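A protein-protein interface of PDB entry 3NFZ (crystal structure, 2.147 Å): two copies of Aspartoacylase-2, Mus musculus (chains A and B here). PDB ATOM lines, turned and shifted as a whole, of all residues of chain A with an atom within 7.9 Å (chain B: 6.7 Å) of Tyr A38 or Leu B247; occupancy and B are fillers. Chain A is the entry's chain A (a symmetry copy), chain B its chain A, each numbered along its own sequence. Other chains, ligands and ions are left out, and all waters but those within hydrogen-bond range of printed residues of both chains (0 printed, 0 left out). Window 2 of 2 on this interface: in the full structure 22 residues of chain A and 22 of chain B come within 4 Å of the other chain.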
ATOM      1  N   GLY A  27      22.011 -18.508   1.247  1.00  0.00           N
ATOM      2  CA  GLY A  27      21.951 -19.501   2.309  1.00  0.00           C
ATOM      3  C   GLY A  27      20.514 -19.958   2.459  1.00  0.00           C
ATOM      4  O   GLY A  27      19.611 -19.270   1.993  1.00  0.00           O
ATOM      5  N   GLY A  28      20.291 -21.114   3.086  1.00  0.00           N
ATOM      6  CA  GLY A  28      18.937 -21.618   3.271  1.00  0.00           C
ATOM      7  C   GLY A  28      18.200 -21.993   1.988  1.00  0.00           C
ATOM      8  O   GLY A  28      16.971 -21.932   1.932  1.00  0.00           O
ATOM      9  N   GLY A  31      15.934 -25.251   3.849  1.00  0.00           N
ATOM     10  CA  GLY A  31      15.650 -24.501   5.070  1.00  0.00           C
ATOM     11  C   GLY A  31      16.162 -25.102   6.364  1.00  0.00           C
ATOM     12  O   GLY A  31      16.167 -24.421   7.391  1.00  0.00           O
ATOM     13  N   GLU A  33      19.290 -26.590   6.612  1.00  0.00           N
ATOM     14  CA  GLU A  33      20.752 -26.660   6.556  1.00  0.00           C
ATOM     15  C   GLU A  33      21.325 -25.418   7.221  1.00  0.00           C
ATOM     16  O   GLU A  33      21.387 -24.336   6.625  1.00  0.00           O
ATOM     17  CB  GLU A  33      21.229 -26.878   5.119  1.00  0.00           C
ATOM     18  CG  GLU A  33      20.965 -28.329   4.675  1.00  0.00           C
ATOM     19  CD  GLU A  33      21.271 -28.600   3.216  1.00  0.00           C
ATOM     20  OE1 GLU A  33      21.947 -27.773   2.564  1.00  0.00           O
ATOM     21  OE2 GLU A  33      20.823 -29.659   2.722  1.00  0.00           O
ATOM     22  N   MET A  34      21.713 -25.587   8.481  1.00  0.00           N
ATOM     23  CA  MET A  34      21.797 -24.460   9.408  1.00  0.00           C
ATOM     24  C   MET A  34      22.937 -23.454   9.226  1.00  0.00           C
ATOM     25  O   MET A  34      22.781 -22.293   9.619  1.00  0.00           O
ATOM     26  CB  MET A  34      21.749 -24.958  10.863  1.00  0.00           C
ATOM     27  CG  MET A  34      20.536 -25.855  11.163  1.00  0.00           C
ATOM     28  SD  MET A  34      18.961 -24.967  10.961  1.00  0.00           S
ATOM     29  CE  MET A  34      18.715 -24.443  12.667  1.00  0.00           C
ATOM     30  N   CYS A  35      24.080 -23.864   8.675  1.00  0.00           N
ATOM     31  CA  CYS A  35      25.171 -22.884   8.505  1.00  0.00           C
ATOM     32  C   CYS A  35      24.735 -21.755   7.589  1.00  0.00           C
ATOM     33  O   CYS A  35      24.847 -20.578   7.943  1.00  0.00           O
ATOM     34  CB  CYS A  35      26.453 -23.520   7.960  1.00  0.00           C
ATOM     35  SG  CYS A  35      27.235 -24.682   9.120  1.00  0.00           S
ATOM     36  N   GLY A  36      24.233 -22.121   6.412  1.00  0.00           N
ATOM     37  CA  GLY A  36      23.832 -21.140   5.421  1.00  0.00           C
ATOM     38  C   GLY A  36      22.656 -20.309   5.897  1.00  0.00           C
ATOM     39  O   GLY A  36      22.594 -19.114   5.628  1.00  0.00           O
ATOM     40  N   VAL A  37      21.713 -20.948   6.595  1.00  0.00           N
ATOM     41  CA  VAL A  37      20.564 -20.241   7.149  1.00  0.00           C
ATOM     42  C   VAL A  37      21.050 -19.114   8.066  1.00  0.00           C
ATOM     43  O   VAL A  37      20.662 -17.950   7.913  1.00  0.00           O
ATOM     44  CB  VAL A  37      19.615 -21.200   7.943  1.00  0.00           C
ATOM     45  CG1 VAL A  37      18.739 -20.415   8.913  1.00  0.00           C
ATOM     46  CG2 VAL A  37      18.765 -22.032   6.996  1.00  0.00           C
ATOM     47  N   TYR A  38      21.925 -19.454   9.006  1.00  0.00           N
ATOM     48  CA  TYR A  38      22.329 -18.477  10.013  1.00  0.00           C
ATOM     49  C   TYR A  38      23.374 -17.480   9.517  1.00  0.00           C
ATOM     50  O   TYR A  38      23.378 -16.331   9.942  1.00  0.00           O
ATOM     51  CB  TYR A  38      22.716 -19.168  11.347  1.00  0.00           C
ATOM     52  CG  TYR A  38      21.464 -19.441  12.149  1.00  0.00           C
ATOM     53  CD1 TYR A  38      20.798 -18.399  12.794  1.00  0.00           C
ATOM     54  CD2 TYR A  38      20.886 -20.708  12.176  1.00  0.00           C
ATOM     55  CE1 TYR A  38      19.621 -18.616  13.493  1.00  0.00           C
ATOM     56  CE2 TYR A  38      19.704 -20.938  12.878  1.00  0.00           C
ATOM     57  CZ  TYR A  38      19.082 -19.889  13.532  1.00  0.00           C
ATOM     58  OH  TYR A  38      17.916 -20.103  14.227  1.00  0.00           O
ATOM     59  N   LEU A  39      24.235 -17.907   8.597  1.00  0.00           N
ATOM     60  CA  LEU A  39      25.125 -16.962   7.926  1.00  0.00           C
ATOM     61  C   LEU A  39      24.328 -15.931   7.126  1.00  0.00           C
ATOM     62  O   LEU A  39      24.583 -14.738   7.250  1.00  0.00           O
ATOM     63  CB  LEU A  39      26.162 -17.677   7.050  1.00  0.00           C
ATOM     64  CG  LEU A  39      27.268 -18.386   7.850  1.00  0.00           C
ATOM     65  CD1 LEU A  39      28.073 -19.325   6.962  1.00  0.00           C
ATOM     66  CD2 LEU A  39      28.186 -17.360   8.538  1.00  0.00           C
ATOM     67  N   ALA A  40      23.358 -16.385   6.330  1.00  0.00           N
ATOM     68  CA  ALA A  40      22.517 -15.462   5.560  1.00  0.00           C
ATOM     69  C   ALA A  40      21.776 -14.485   6.470  1.00  0.00           C
ATOM     70  O   ALA A  40      21.750 -13.284   6.199  1.00  0.00           O
ATOM     71  CB  ALA A  40      21.520 -16.222   4.683  1.00  0.00           C
ATOM     72  N   ARG A  41      21.171 -14.997   7.541  1.00  0.00           N
ATOM     73  CA  ARG A  41      20.469 -14.135   8.503  1.00  0.00           C
ATOM     74  C   ARG A  41      21.432 -13.156   9.178  1.00  0.00           C
ATOM     75  O   ARG A  41      21.125 -11.979   9.358  1.00  0.00           O
ATOM     76  CB  ARG A  41      19.750 -14.969   9.567  1.00  0.00           C
ATOM     77  CG  ARG A  41      18.439 -15.595   9.113  1.00  0.00           C
ATOM     78  CD  ARG A  41      17.970 -16.652  10.116  1.00  0.00           C
ATOM     79  NE  ARG A  41      16.561 -17.004   9.946  1.00  0.00           N
ATOM     80  CZ  ARG A  41      15.925 -17.957  10.633  1.00  0.00           C
ATOM     81  NH1 ARG A  41      16.561 -18.681  11.551  1.00  0.00           N
ATOM     82  NH2 ARG A  41      14.644 -18.189  10.398  1.00  0.00           N
ATOM     83  N   TYR A  42      22.603 -13.648   9.554  1.00  0.00           N
ATOM     84  CA  TYR A  42      23.580 -12.787  10.191  1.00  0.00           C
ATOM     85  C   TYR A  42      24.039 -11.651   9.267  1.00  0.00           C
ATOM     86  O   TYR A  42      24.087 -10.491   9.683  1.00  0.00           O
ATOM     87  CB  TYR A  42      24.772 -13.595  10.673  1.00  0.00           C
ATOM     88  CG  TYR A  42      25.827 -12.749  11.327  1.00  0.00           C
ATOM     89  CD1 TYR A  42      25.729 -12.402  12.670  1.00  0.00           C
ATOM     90  CD2 TYR A  42      26.916 -12.282  10.602  1.00  0.00           C
ATOM     91  CE1 TYR A  42      26.693 -11.618  13.276  1.00  0.00           C
ATOM     92  CE2 TYR A  42      27.889 -11.499  11.201  1.00  0.00           C
ATOM     93  CZ  TYR A  42      27.773 -11.174  12.539  1.00  0.00           C
ATOM     94  OH  TYR A  42      28.740 -10.397  13.144  1.00  0.00           O
ATOM     95  N   TRP A  43      24.350 -11.990   8.015  1.00  0.00           N
ATOM     96  CA  TRP A  43      24.880 -11.021   7.053  1.00  0.00           C
ATOM     97  C   TRP A  43      23.821 -10.025   6.596  1.00  0.00           C
ATOM     98  O   TRP A  43      24.151  -8.913   6.191  1.00  0.00           O
ATOM     99  CB  TRP A  43      25.476 -11.716   5.817  1.00  0.00           C
ATOM    100  CG  TRP A  43      26.755 -12.456   6.069  1.00  0.00           C
ATOM    101  CD1 TRP A  43      27.770 -12.090   6.917  1.00  0.00           C
ATOM    102  CD2 TRP A  43      27.168 -13.687   5.456  1.00  0.00           C
ATOM    103  NE1 TRP A  43      28.781 -13.024   6.871  1.00  0.00           N
ATOM    104  CE2 TRP A  43      28.431 -14.016   5.985  1.00  0.00           C
ATOM    105  CE3 TRP A  43      26.585 -14.545   4.517  1.00  0.00           C
ATOM    106  CZ2 TRP A  43      29.132 -15.159   5.596  1.00  0.00           C
ATOM    107  CZ3 TRP A  43      27.283 -15.686   4.136  1.00  0.00           C
ATOM    108  CH2 TRP A  43      28.541 -15.977   4.673  1.00  0.00           C
ATOM    109  N   LEU A  44      22.554 -10.435   6.624  1.00  0.00           N
ATOM    110  CA  LEU A  44      21.476  -9.515   6.289  1.00  0.00           C
ATOM    111  C   LEU A  44      21.417  -8.423   7.359  1.00  0.00           C
ATOM    112  O   LEU A  44      21.103  -7.271   7.051  1.00  0.00           O
ATOM    113  CB  LEU A  44      20.129 -10.233   6.164  1.00  0.00           C
ATOM    114  CG  LEU A  44      19.864 -11.038   4.884  1.00  0.00           C
ATOM    115  CD1 LEU A  44      18.671 -11.961   5.100  1.00  0.00           C
ATOM    116  CD2 LEU A  44      19.655 -10.123   3.652  1.00  0.00           C
ATOM    117  N   GLN A  45      21.736  -8.785   8.603  1.00  0.00           N
ATOM    118  CA  GLN A  45      21.840  -7.798   9.683  1.00  0.00           C
ATOM    119  C   GLN A  45      23.186  -7.093   9.665  1.00  0.00           C
ATOM    120  O   GLN A  45      23.283  -5.939  10.074  1.00  0.00           O
ATOM    121  CB  GLN A  45      21.639  -8.434  11.062  1.00  0.00           C
ATOM    122  CG  GLN A  45      20.256  -9.003  11.273  1.00  0.00           C
ATOM    123  CD  GLN A  45      19.168  -8.024  10.875  1.00  0.00           C
ATOM    124  OE1 GLN A  45      19.135  -6.912  11.450  1.00  0.00           O
ATOM    125  NE2 GLN A  45      18.349  -8.366   9.987  1.00  0.00           N
ATOM    126  N   LEU A  61      18.587 -15.063   1.574  1.00  0.00           N
ATOM    127  CA  LEU A  61      17.976 -16.253   2.152  1.00  0.00           C
ATOM    128  C   LEU A  61      17.103 -16.877   1.060  1.00  0.00           C
ATOM    129  O   LEU A  61      16.033 -16.349   0.734  1.00  0.00           O
ATOM    130  CB  LEU A  61      17.143 -15.874   3.381  1.00  0.00           C
ATOM    131  CG  LEU A  61      16.605 -17.030   4.231  1.00  0.00           C
ATOM    132  CD1 LEU A  61      17.742 -17.847   4.821  1.00  0.00           C
ATOM    133  CD2 LEU A  61      15.706 -16.470   5.331  1.00  0.00           C
ATOM    134  N   THR A  67      12.930 -22.203   5.517  1.00  0.00           N
ATOM    135  CA  THR A  67      13.780 -21.794   6.625  1.00  0.00           C
ATOM    136  C   THR A  67      12.954 -21.525   7.884  1.00  0.00           C
ATOM    137  O   THR A  67      13.316 -21.966   8.980  1.00  0.00           O
ATOM    138  CB  THR A  67      14.630 -20.553   6.260  1.00  0.00           C
ATOM    139  OG1 THR A  67      15.572 -20.897   5.227  1.00  0.00           O
ATOM    140  CG2 THR A  67      15.385 -20.045   7.496  1.00  0.00           C
ATOM    141  N   CYS A  70      11.993 -24.592   9.345  1.00  0.00           N
ATOM    142  CA  CYS A  70      13.143 -25.479   9.492  1.00  0.00           C
ATOM    143  C   CYS A  70      12.939 -26.837   8.807  1.00  0.00           C
ATOM    144  O   CYS A  70      13.030 -27.881   9.441  1.00  0.00           O
ATOM    145  CB  CYS A  70      13.529 -25.687  10.965  1.00  0.00           C
ATOM    146  SG  CYS A  70      15.183 -26.458  11.149  1.00  0.00           S
ATOM    147  N   LEU A 124      25.341 -22.009  -0.294  1.00  0.00           N
ATOM    148  CA  LEU A 124      25.849 -22.732   0.878  1.00  0.00           C
ATOM    149  C   LEU A 124      24.989 -23.942   1.287  1.00  0.00           C
ATOM    150  O   LEU A 124      23.772 -23.831   1.444  1.00  0.00           O
ATOM    151  CB  LEU A 124      25.985 -21.772   2.068  1.00  0.00           C
ATOM    152  CG  LEU A 124      26.649 -20.433   1.739  1.00  0.00           C
ATOM    153  CD1 LEU A 124      26.495 -19.429   2.904  1.00  0.00           C
ATOM    154  CD2 LEU A 124      28.111 -20.645   1.387  1.00  0.00           C
ATOM    155  N   ASN A 126      24.746 -27.797   3.708  1.00  0.00           N
ATOM    156  CA  ASN A 126      25.257 -28.798   4.639  1.00  0.00           C
ATOM    157  C   ASN A 126      24.793 -30.171   4.216  1.00  0.00           C
ATOM    158  O   ASN A 126      23.800 -30.304   3.500  1.00  0.00           O
ATOM    159  CB  ASN A 126      24.781 -28.522   6.064  1.00  0.00           C
ATOM    160  CG  ASN A 126      25.400 -27.268   6.639  1.00  0.00           C
ATOM    161  OD1 ASN A 126      24.706 -26.289   6.866  1.00  0.00           O
ATOM    162  ND2 ASN A 126      26.728 -27.291   6.874  1.00  0.00           N
ATOM    163  N   GLY A 193      18.849 -29.208  10.965  1.00  0.00           N
ATOM    164  CA  GLY A 193      18.292 -28.524  12.123  1.00  0.00           C
ATOM    165  C   GLY A 193      19.267 -28.357  13.285  1.00  0.00           C
ATOM    166  O   GLY A 193      18.881 -27.914  14.359  1.00  0.00           O
ATOM    167  N   VAL A 194      20.532 -28.721  13.087  1.00  0.00           N
ATOM    168  CA  VAL A 194      21.543 -28.488  14.122  1.00  0.00           C
ATOM    169  C   VAL A 194      22.584 -27.512  13.604  1.00  0.00           C
ATOM    170  O   VAL A 194      23.058 -27.655  12.474  1.00  0.00           O
ATOM    171  CB  VAL A 194      22.249 -29.799  14.555  1.00  0.00           C
ATOM    172  CG1 VAL A 194      23.425 -29.496  15.461  1.00  0.00           C
ATOM    173  CG2 VAL A 194      21.262 -30.755  15.249  1.00  0.00           C
ATOM    174  N   LEU A 195      22.918 -26.504  14.412  1.00  0.00           N
ATOM    175  CA  LEU A 195      24.033 -25.609  14.087  1.00  0.00           C
ATOM    176  C   LEU A 195      25.246 -25.912  14.964  1.00  0.00           C
ATOM    177  O   LEU A 195      25.215 -25.708  16.186  1.00  0.00           O
ATOM    178  CB  LEU A 195      23.625 -24.132  14.243  1.00  0.00           C
ATOM    179  CG  LEU A 195      24.688 -23.077  13.900  1.00  0.00           C
ATOM    180  CD1 LEU A 195      25.154 -23.216  12.449  1.00  0.00           C
ATOM    181  CD2 LEU A 195      24.163 -21.663  14.133  1.00  0.00           C
ATOM    182  N   PHE A 200      30.027 -23.700  11.434  1.00  0.00           N
ATOM    183  CA  PHE A 200      29.617 -22.318  11.199  1.00  0.00           C
ATOM    184  C   PHE A 200      30.849 -21.431  10.967  1.00  0.00           C
ATOM    185  O   PHE A 200      30.914 -20.702   9.977  1.00  0.00           O
ATOM    186  CB  PHE A 200      28.812 -21.800  12.395  1.00  0.00           C
ATOM    187  CG  PHE A 200      28.352 -20.365  12.260  1.00  0.00           C
ATOM    188  CD1 PHE A 200      27.237 -20.047  11.497  1.00  0.00           C
ATOM    189  CD2 PHE A 200      29.017 -19.339  12.928  1.00  0.00           C
ATOM    190  CE1 PHE A 200      26.787 -18.726  11.393  1.00  0.00           C
ATOM    191  CE2 PHE A 200      28.578 -18.017  12.825  1.00  0.00           C
ATOM    192  CZ  PHE A 200      27.461 -17.709  12.056  1.00  0.00           C
ATOM    193  N   ASP B 238      19.039 -22.561  27.863  1.00  0.00           N
ATOM    194  CA  ASP B 238      18.621 -22.230  26.509  1.00  0.00           C
ATOM    195  C   ASP B 238      19.779 -21.671  25.681  1.00  0.00           C
ATOM    196  O   ASP B 238      20.782 -21.207  26.233  1.00  0.00           O
ATOM    197  CB  ASP B 238      17.496 -21.197  26.559  1.00  0.00           C
ATOM    198  CG  ASP B 238      16.896 -20.922  25.190  1.00  0.00           C
ATOM    199  OD1 ASP B 238      17.126 -21.723  24.252  1.00  0.00           O
ATOM    200  OD2 ASP B 238      16.183 -19.909  25.053  1.00  0.00           O
ATOM    201  N   PHE B 239      19.639 -21.722  24.357  1.00  0.00           N
ATOM    202  CA  PHE B 239      20.574 -21.063  23.460  1.00  0.00           C
ATOM    203  C   PHE B 239      20.595 -19.570  23.752  1.00  0.00           C
ATOM    204  O   PHE B 239      19.581 -19.007  24.170  1.00  0.00           O
ATOM    205  CB  PHE B 239      20.157 -21.261  22.006  1.00  0.00           C
ATOM    206  CG  PHE B 239      20.364 -22.648  21.503  1.00  0.00           C
ATOM    207  CD1 PHE B 239      21.569 -23.015  20.923  1.00  0.00           C
ATOM    208  CD2 PHE B 239      19.352 -23.594  21.604  1.00  0.00           C
ATOM    209  CE1 PHE B 239      21.762 -24.304  20.453  1.00  0.00           C
ATOM    210  CE2 PHE B 239      19.539 -24.884  21.140  1.00  0.00           C
ATOM    211  CZ  PHE B 239      20.744 -25.239  20.559  1.00  0.00           C
ATOM    212  N   PRO B 240      21.745 -18.920  23.514  1.00  0.00           N
ATOM    213  CA  PRO B 240      21.787 -17.460  23.668  1.00  0.00           C
ATOM    214  C   PRO B 240      20.898 -16.863  22.593  1.00  0.00           C
ATOM    215  O   PRO B 240      20.965 -17.322  21.448  1.00  0.00           O
ATOM    216  CB  PRO B 240      23.254 -17.100  23.369  1.00  0.00           C
ATOM    217  CG  PRO B 240      23.976 -18.393  23.097  1.00  0.00           C
ATOM    218  CD  PRO B 240      22.941 -19.456  22.841  1.00  0.00           C
ATOM    219  N   ARG B 241      20.086 -15.869  22.929  1.00  0.00           N
ATOM    220  CA  ARG B 241      19.164 -15.305  21.941  1.00  0.00           C
ATOM    221  C   ARG B 241      19.195 -13.787  21.861  1.00  0.00           C
ATOM    222  O   ARG B 241      19.662 -13.109  22.782  1.00  0.00           O
ATOM    223  CB  ARG B 241      17.734 -15.796  22.194  1.00  0.00           C
ATOM    224  CG  ARG B 241      17.596 -17.309  22.022  1.00  0.00           C
ATOM    225  CD  ARG B 241      16.179 -17.822  22.247  1.00  0.00           C
ATOM    226  NE  ARG B 241      16.181 -19.281  22.304  1.00  0.00           N
ATOM    227  CZ  ARG B 241      15.995 -20.076  21.256  1.00  0.00           C
ATOM    228  NH1 ARG B 241      15.751 -19.562  20.056  1.00  0.00           N
ATOM    229  NH2 ARG B 241      16.032 -21.392  21.412  1.00  0.00           N
ATOM    230  N   THR B 242      18.717 -13.268  20.734  1.00  0.00           N
ATOM    231  CA  THR B 242      18.475 -11.841  20.578  1.00  0.00           C
ATOM    232  C   THR B 242      17.191 -11.503  21.315  1.00  0.00           C
ATOM    233  O   THR B 242      16.504 -12.403  21.808  1.00  0.00           O
ATOM    234  CB  THR B 242      18.264 -11.475  19.109  1.00  0.00           C
ATOM    235  OG1 THR B 242      17.123 -12.187  18.608  1.00  0.00           O
ATOM    236  CG2 THR B 242      19.490 -11.851  18.284  1.00  0.00           C
ATOM    237  N   GLY B 245      14.392 -13.519  20.235  1.00  0.00           N
ATOM    238  CA  GLY B 245      14.456 -14.953  20.459  1.00  0.00           C
ATOM    239  C   GLY B 245      15.063 -15.739  19.310  1.00  0.00           C
ATOM    240  O   GLY B 245      14.915 -16.960  19.244  1.00  0.00           O
ATOM    241  N   ASP B 246      15.733 -15.046  18.393  1.00  0.00           N
ATOM    242  CA  ASP B 246      16.500 -15.712  17.344  1.00  0.00           C
ATOM    243  C   ASP B 246      17.849 -16.078  17.944  1.00  0.00           C
ATOM    244  O   ASP B 246      18.343 -15.365  18.817  1.00  0.00           O
ATOM    245  CB  ASP B 246      16.726 -14.780  16.150  1.00  0.00           C
ATOM    246  CG  ASP B 246      15.525 -13.900  15.850  1.00  0.00           C
ATOM    247  OD1 ASP B 246      14.455 -14.452  15.516  1.00  0.00           O
ATOM    248  OD2 ASP B 246      15.659 -12.654  15.935  1.00  0.00           O
ATOM    249  N   LEU B 247      18.453 -17.172  17.486  1.00  0.00           N
ATOM    250  CA  LEU B 247      19.772 -17.539  17.980  1.00  0.00           C
ATOM    251  C   LEU B 247      20.729 -16.362  17.850  1.00  0.00           C
ATOM    252  O   LEU B 247      20.760 -15.697  16.821  1.00  0.00           O
ATOM    253  CB  LEU B 247      20.359 -18.712  17.199  1.00  0.00           C
ATOM    254  CG  LEU B 247      19.752 -20.109  17.229  1.00  0.00           C
ATOM    255  CD1 LEU B 247      20.735 -21.091  16.588  1.00  0.00           C
ATOM    256  CD2 LEU B 247      19.411 -20.553  18.629  1.00  0.00           C
ATOM    257  N   ALA B 248      21.523 -16.125  18.885  1.00  0.00           N
ATOM    258  CA  ALA B 248      22.625 -15.170  18.794  1.00  0.00           C
ATOM    259  C   ALA B 248      23.960 -15.925  18.798  1.00  0.00           C
ATOM    260  O   ALA B 248      25.033 -15.324  18.712  1.00  0.00           O
ATOM    261  CB  ALA B 248      22.566 -14.174  19.949  1.00  0.00           C
ATOM    262  N   GLY B 249      23.881 -17.251  18.907  1.00  0.00           N
ATOM    263  CA  GLY B 249      25.063 -18.095  18.850  1.00  0.00           C
ATOM    264  C   GLY B 249      24.685 -19.549  19.012  1.00  0.00           C
ATOM    265  O   GLY B 249      23.500 -19.882  19.009  1.00  0.00           O
ATOM    266  N   THR B 250      25.675 -20.423  19.165  1.00  0.00           N
ATOM    267  CA  THR B 250      25.363 -21.829  19.394  1.00  0.00           C
ATOM    268  C   THR B 250      26.316 -22.497  20.393  1.00  0.00           C
ATOM    269  O   THR B 250      27.191 -21.840  20.978  1.00  0.00           O
ATOM    270  CB  THR B 250      25.296 -22.627  18.064  1.00  0.00           C
ATOM    271  OG1 THR B 250      24.712 -23.914  18.303  1.00  0.00           O
ATOM    272  CG2 THR B 250      26.694 -22.772  17.417  1.00  0.00           C
ATOM    273  N   PHE B 273      27.708 -15.385  17.566  1.00  0.00           N
ATOM    274  CA  PHE B 273      28.077 -15.043  16.194  1.00  0.00           C
ATOM    275  C   PHE B 273      29.007 -13.828  16.161  1.00  0.00           C
ATOM    276  O   PHE B 273      29.803 -13.668  15.235  1.00  0.00           O
ATOM    277  CB  PHE B 273      26.839 -14.816  15.322  1.00  0.00           C
ATOM    278  CG  PHE B 273      25.887 -15.987  15.304  1.00  0.00           C
ATOM    279  CD1 PHE B 273      26.370 -17.290  15.295  1.00  0.00           C
ATOM    280  CD2 PHE B 273      24.510 -15.782  15.309  1.00  0.00           C
ATOM    281  CE1 PHE B 273      25.495 -18.382  15.287  1.00  0.00           C
ATOM    282  CE2 PHE B 273      23.615 -16.864  15.305  1.00  0.00           C
ATOM    283  CZ  PHE B 273      24.113 -18.170  15.287  1.00  0.00           C
ATOM    284  N   TYR B 297      15.722 -27.149  19.869  1.00  0.00           N
ATOM    285  CA  TYR B 297      15.816 -25.728  19.511  1.00  0.00           C
ATOM    286  C   TYR B 297      14.489 -25.027  19.832  1.00  0.00           C
ATOM    287  O   TYR B 297      14.463 -24.030  20.555  1.00  0.00           O
ATOM    288  CB  TYR B 297      16.173 -25.553  18.026  1.00  0.00           C
ATOM    289  CG  TYR B 297      17.661 -25.698  17.728  1.00  0.00           C
ATOM    290  CD1 TYR B 297      18.335 -26.888  17.977  1.00  0.00           C
ATOM    291  CD2 TYR B 297      18.385 -24.641  17.195  1.00  0.00           C
ATOM    292  CE1 TYR B 297      19.687 -27.017  17.704  1.00  0.00           C
ATOM    293  CE2 TYR B 297      19.734 -24.756  16.935  1.00  0.00           C
ATOM    294  CZ  TYR B 297      20.379 -25.939  17.178  1.00  0.00           C
ATOM    295  OH  TYR B 297      21.728 -26.026  16.921  1.00  0.00           O
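The backbone carbonyl oxygen of Leu A195 is in hydrogen-bond range of the side-chain hydroxyl of Thr B250.
The side-chain hydroxyl of Tyr B297 lies within hydrogen-bond range of the backbone NH of Leu A195.
O of Tyr B297 is in hydrogen-bond range of NH2 of Arg B241 (3.2 Å).
The backbone carbonyl oxygen (O) of Ala B248 is in hydrogen-bond range of the backbone NH (N) of Phe B273 (2.9 Å).
The side-chain sulfur (SG) of Cys A35 lies within hydrogen-bond range of the backbone NH (N) of Phe A200 (3.8 Å).
The guanidinium group (NH1) of Arg A41 lies within hydrogen-bond range of the side-chain hydroxyl (OH) of Tyr A38, at 3.3 Å.
Among the printed residues, merely in contact across the chains: Phe A200 with Phe B273 (3.4 Å), Tyr A38 with Leu B247 (3.5 Å), Gly A193 with Tyr B297 (3.6 Å), Leu A195 with Phe B273 (3.7 Å), Val A194 with Tyr B297 (3.7 Å) and Tyr A42 with Phe B273 (3.8 Å).
Tyr A38 touches just one residue of chain B: Leu B247 (3.5 Å).
Leu B247 touches one residue of chain A.
Of the printed residues of chain B, Val A194 touches Tyr B297.
Printed residues of chain A within 4 Å of Thr B250: Leu A195.
Of the printed residues of chain B, Tyr A42 touches Phe B273 (3.8 Å).
Of the printed residues of chain A, Tyr B297 touches Gly A193, Val A194 and Leu A195.
The nearest residue of chain B that does not touch Tyr A38 is Phe B273 (4.1 Å).
Printed residues of chain B that touch a printed residue of chain A: Leu B247, Thr B250, Phe B273 and Tyr B297.
Of the 25 printed residues of chain A, 6 touch a printed residue of chain B.
Among the printed residues, 8 pairs touch across the chains.
Among the printed residues, no Asp or Glu carboxylate lies within 4 Å of a Lys or Arg side-chain nitrogen of the other chain.
No position is printed for both chains.
Of the 8 pairs that touch across the chains among the printed residues, none has its exchanged pair printed and touching as well.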
